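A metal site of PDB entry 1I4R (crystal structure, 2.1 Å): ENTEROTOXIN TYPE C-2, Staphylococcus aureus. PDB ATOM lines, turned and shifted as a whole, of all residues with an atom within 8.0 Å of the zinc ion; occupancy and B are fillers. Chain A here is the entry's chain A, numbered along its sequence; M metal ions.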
ATOM      1  N   ALA A  35     -31.270  -2.086  29.299  1.00  0.00           N
ATOM      2  CA  ALA A  35     -30.471  -1.829  30.490  1.00  0.00           C
ATOM      3  C   ALA A  35     -29.350  -0.840  30.168  1.00  0.00           C
ATOM      4  O   ALA A  35     -28.834  -0.814  29.049  1.00  0.00           O
ATOM      5  CB  ALA A  35     -29.897  -3.132  31.027  1.00  0.00           C
ATOM      6  N   THR A  36     -28.991  -0.014  31.144  1.00  0.00           N
ATOM      7  CA  THR A  36     -27.912   0.930  30.914  1.00  0.00           C
ATOM      8  C   THR A  36     -26.870   0.867  32.020  1.00  0.00           C
ATOM      9  O   THR A  36     -27.184   0.746  33.207  1.00  0.00           O
ATOM     10  CB  THR A  36     -28.402   2.413  30.759  1.00  0.00           C
ATOM     11  OG1 THR A  36     -27.804   3.239  31.750  1.00  0.00           O
ATOM     12  CG2 THR A  36     -29.878   2.503  30.909  1.00  0.00           C
ATOM     13  N   LYS A  37     -25.613   0.904  31.604  1.00  0.00           N
ATOM     14  CA  LYS A  37     -24.479   0.877  32.518  1.00  0.00           C
ATOM     15  C   LYS A  37     -24.422  -0.328  33.448  1.00  0.00           C
ATOM     16  O   LYS A  37     -24.309  -0.189  34.665  1.00  0.00           O
ATOM     17  CB  LYS A  37     -24.475   2.173  33.329  1.00  0.00           C
ATOM     18  CG  LYS A  37     -24.283   3.395  32.450  1.00  0.00           C
ATOM     19  CD  LYS A  37     -24.358   4.690  33.248  1.00  0.00           C
ATOM     20  CE  LYS A  37     -23.219   4.790  34.242  1.00  0.00           C
ATOM     21  NZ  LYS A  37     -23.307   6.029  35.035  1.00  0.00           N
ATOM     22  N   VAL A  38     -24.489  -1.522  32.872  1.00  0.00           N
ATOM     23  CA  VAL A  38     -24.406  -2.757  33.657  1.00  0.00           C
ATOM     24  C   VAL A  38     -23.106  -3.461  33.303  1.00  0.00           C
ATOM     25  O   VAL A  38     -22.488  -3.165  32.279  1.00  0.00           O
ATOM     26  CB  VAL A  38     -25.611  -3.700  33.375  1.00  0.00           C
ATOM     27  CG1 VAL A  38     -26.881  -3.128  33.976  1.00  0.00           C
ATOM     28  CG2 VAL A  38     -25.777  -3.905  31.874  1.00  0.00           C
ATOM     29  N   VAL A  81     -18.495  -1.632  31.120  1.00  0.00           N
ATOM     30  CA  VAL A  81     -19.751  -1.045  31.569  1.00  0.00           C
ATOM     31  C   VAL A  81     -20.456  -0.861  30.232  1.00  0.00           C
ATOM     32  O   VAL A  81     -20.020  -0.065  29.412  1.00  0.00           O
ATOM     33  CB  VAL A  81     -19.558   0.332  32.252  1.00  0.00           C
ATOM     34  CG1 VAL A  81     -20.918   0.926  32.598  1.00  0.00           C
ATOM     35  CG2 VAL A  81     -18.712   0.191  33.524  1.00  0.00           C
ATOM     36  N   VAL A  82     -21.538  -1.604  30.021  1.00  0.00           N
ATOM     37  CA  VAL A  82     -22.258  -1.544  28.755  1.00  0.00           C
ATOM     38  C   VAL A  82     -23.745  -1.245  28.887  1.00  0.00           C
ATOM     39  O   VAL A  82     -24.301  -1.256  29.989  1.00  0.00           O
ATOM     40  CB  VAL A  82     -22.145  -2.892  28.004  1.00  0.00           C
ATOM     41  CG1 VAL A  82     -20.674  -3.295  27.864  1.00  0.00           C
ATOM     42  CG2 VAL A  82     -22.895  -3.965  28.764  1.00  0.00           C
ATOM     43  N   ASP A  83     -24.382  -0.966  27.747  1.00  0.00           N
ATOM     44  CA  ASP A  83     -25.820  -0.757  27.700  1.00  0.00           C
ATOM     45  C   ASP A  83     -26.300  -1.974  26.912  1.00  0.00           C
ATOM     46  O   ASP A  83     -25.562  -2.513  26.087  1.00  0.00           O
ATOM     47  CB  ASP A  83     -26.190   0.526  26.947  1.00  0.00           C
ATOM     48  CG  ASP A  83     -25.700   1.778  27.644  1.00  0.00           C
ATOM     49  OD1 ASP A  83     -25.695   1.795  28.894  1.00  0.00           O
ATOM     50  OD2 ASP A  83     -25.336   2.750  26.942  1.00  0.00           O
ATOM     51  N   VAL A  84     -27.534  -2.408  27.171  1.00  0.00           N
ATOM     52  CA  VAL A  84     -28.094  -3.578  26.511  1.00  0.00           C
ATOM     53  C   VAL A  84     -29.442  -3.321  25.846  1.00  0.00           C
ATOM     54  O   VAL A  84     -30.285  -2.599  26.371  1.00  0.00           O
ATOM     55  CB  VAL A  84     -28.268  -4.739  27.530  1.00  0.00           C
ATOM     56  CG1 VAL A  84     -28.688  -6.008  26.811  1.00  0.00           C
ATOM     57  CG2 VAL A  84     -26.965  -4.963  28.304  1.00  0.00           C
ATOM     58  N   THR A 116     -23.388  -2.768  23.823  1.00  0.00           N
ATOM     59  CA  THR A 116     -22.531  -1.671  23.395  1.00  0.00           C
ATOM     60  C   THR A 116     -21.912  -0.988  24.606  1.00  0.00           C
ATOM     61  O   THR A 116     -22.543  -0.889  25.660  1.00  0.00           O
ATOM     62  CB  THR A 116     -23.329  -0.620  22.566  1.00  0.00           C
ATOM     63  OG1 THR A 116     -24.576  -0.336  23.204  1.00  0.00           O
ATOM     64  CG2 THR A 116     -23.592  -1.125  21.167  1.00  0.00           C
ATOM     65  N   LYS A 117     -20.675  -0.526  24.476  1.00  0.00           N
ATOM     66  CA  LYS A 117     -20.038   0.161  25.605  1.00  0.00           C
ATOM     67  C   LYS A 117     -20.804   1.458  25.860  1.00  0.00           C
ATOM     68  O   LYS A 117     -21.260   2.113  24.926  1.00  0.00           O
ATOM     69  CB  LYS A 117     -18.582   0.482  25.272  1.00  0.00           C
ATOM     70  CG  LYS A 117     -17.738  -0.736  24.909  1.00  0.00           C
ATOM     71  CD  LYS A 117     -16.361  -0.304  24.402  1.00  0.00           C
ATOM     72  CE  LYS A 117     -15.521  -1.484  23.947  1.00  0.00           C
ATOM     73  NZ  LYS A 117     -14.178  -1.037  23.460  1.00  0.00           N
ATOM     74  N   HIS A 118     -20.931   1.825  27.129  1.00  0.00           N
ATOM     75  CA  HIS A 118     -21.652   3.041  27.515  1.00  0.00           C
ATOM     76  C   HIS A 118     -20.827   4.308  27.279  1.00  0.00           C
ATOM     77  O   HIS A 118     -21.273   5.227  26.611  1.00  0.00           O
ATOM     78  CB  HIS A 118     -22.046   2.979  28.984  1.00  0.00           C
ATOM     79  CG  HIS A 118     -22.438   4.295  29.562  1.00  0.00           C
ATOM     80  ND1 HIS A 118     -23.564   4.987  29.165  1.00  0.00           N
ATOM     81  CD2 HIS A 118     -21.853   5.057  30.515  1.00  0.00           C
ATOM     82  CE1 HIS A 118     -23.653   6.115  29.853  1.00  0.00           C
ATOM     83  NE2 HIS A 118     -22.628   6.174  30.679  1.00  0.00           N
ATOM     84  N   GLU A 119     -19.621   4.339  27.835  1.00  0.00           N
ATOM     85  CA  GLU A 119     -18.751   5.494  27.703  1.00  0.00           C
ATOM     86  C   GLU A 119     -18.507   5.922  26.256  1.00  0.00           C
ATOM     87  O   GLU A 119     -18.208   5.100  25.381  1.00  0.00           O
ATOM     88  CB  GLU A 119     -17.381   5.201  28.353  1.00  0.00           C
ATOM     89  CG  GLU A 119     -16.418   6.387  28.311  1.00  0.00           C
ATOM     90  CD  GLU A 119     -15.076   6.072  28.982  1.00  0.00           C
ATOM     91  OE1 GLU A 119     -14.918   4.952  29.517  1.00  0.00           O
ATOM     92  OE2 GLU A 119     -14.185   6.943  28.986  1.00  0.00           O
ATOM     93  N   GLY A 120     -18.623   7.223  26.019  1.00  0.00           N
ATOM     94  CA  GLY A 120     -18.398   7.809  24.708  1.00  0.00           C
ATOM     95  C   GLY A 120     -19.373   7.424  23.602  1.00  0.00           C
ATOM     96  O   GLY A 120     -19.130   7.752  22.446  1.00  0.00           O
ATOM     97  N   ASN A 121     -20.465   6.761  23.951  1.00  0.00           N
ATOM     98  CA  ASN A 121     -21.415   6.333  22.925  1.00  0.00           C
ATOM     99  C   ASN A 121     -22.742   7.102  22.854  1.00  0.00           C
ATOM    100  O   ASN A 121     -23.713   6.626  22.272  1.00  0.00           O
ATOM    101  CB  ASN A 121     -21.712   4.830  23.072  1.00  0.00           C
ATOM    102  CG  ASN A 121     -22.331   4.241  21.829  1.00  0.00           C
ATOM    103  OD1 ASN A 121     -21.862   4.479  20.720  1.00  0.00           O
ATOM    104  ND2 ASN A 121     -23.394   3.463  22.007  1.00  0.00           N
ATOM    105  N   HIS A 122     -22.779   8.285  23.454  1.00  0.00           N
ATOM    106  CA  HIS A 122     -23.999   9.079  23.399  1.00  0.00           C
ATOM    107  C   HIS A 122     -23.743  10.452  22.788  1.00  0.00           C
ATOM    108  O   HIS A 122     -22.595  10.875  22.664  1.00  0.00           O
ATOM    109  CB  HIS A 122     -24.602   9.180  24.802  1.00  0.00           C
ATOM    110  CG  HIS A 122     -25.177   7.891  25.295  1.00  0.00           C
ATOM    111  ND1 HIS A 122     -26.225   7.259  24.654  1.00  0.00           N
ATOM    112  CD2 HIS A 122     -24.834   7.094  26.329  1.00  0.00           C
ATOM    113  CE1 HIS A 122     -26.493   6.125  25.274  1.00  0.00           C
ATOM    114  NE2 HIS A 122     -25.659   5.999  26.295  1.00  0.00           N
ATOM    115  N   ASP A 150     -30.566   6.534  21.158  1.00  0.00           N
ATOM    116  CA  ASP A 150     -29.722   7.488  21.864  1.00  0.00           C
ATOM    117  C   ASP A 150     -28.247   7.102  21.723  1.00  0.00           C
ATOM    118  O   ASP A 150     -27.371   7.736  22.313  1.00  0.00           O
ATOM    119  CB  ASP A 150     -30.104   7.513  23.342  1.00  0.00           C
ATOM    120  CG  ASP A 150     -29.814   6.191  24.023  1.00  0.00           C
ATOM    121  OD1 ASP A 150     -29.943   5.133  23.379  1.00  0.00           O
ATOM    122  OD2 ASP A 150     -29.475   6.203  25.228  1.00  0.00           O
ATOM    123  N   LYS A 151     -27.986   6.057  20.948  1.00  0.00           N
ATOM    124  CA  LYS A 151     -26.626   5.576  20.757  1.00  0.00           C
ATOM    125  C   LYS A 151     -25.997   6.018  19.432  1.00  0.00           C
ATOM    126  O   LYS A 151     -26.660   5.968  18.393  1.00  0.00           O
ATOM    127  CB  LYS A 151     -26.593   4.050  20.835  1.00  0.00           C
ATOM    128  CG  LYS A 151     -27.119   3.478  22.142  1.00  0.00           C
ATOM    129  CD  LYS A 151     -27.051   1.969  22.114  1.00  0.00           C
ATOM    130  CE  LYS A 151     -27.663   1.367  23.368  1.00  0.00           C
ATOM    131  NZ  LYS A 151     -29.140   1.504  23.370  1.00  0.00           N
HETATM  132 ZN    ZN M   1     -25.227   4.487  27.820  1.00  0.00          ZN
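OD1 of Asp 83 sits at hydrogen-bond distance from N of Lys 37, 2.9 Å away. The backbone NH (N) of Asp 83 lies within hydrogen-bond range of the backbone carbonyl oxygen (O) of Thr 116, at 2.8 Å. The backbone carbonyl oxygen (O) of Asp 150 sits at hydrogen-bond distance from a ring nitrogen (ND1) of His 122, at 2.6 Å. N of His 118 lies within hydrogen-bond range of O of Val 81.
Three residues have an atom within 4 Å of the zinc ion: Asp 83, His 118 and His 122.
The zinc ion is bound by OD2 of Asp 83 (1.9 Å), NE2 of His 122 (2.2 Å) and ND1 of His 118 (2.2 Å). The zinc ion has three donor atoms within binding distance.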
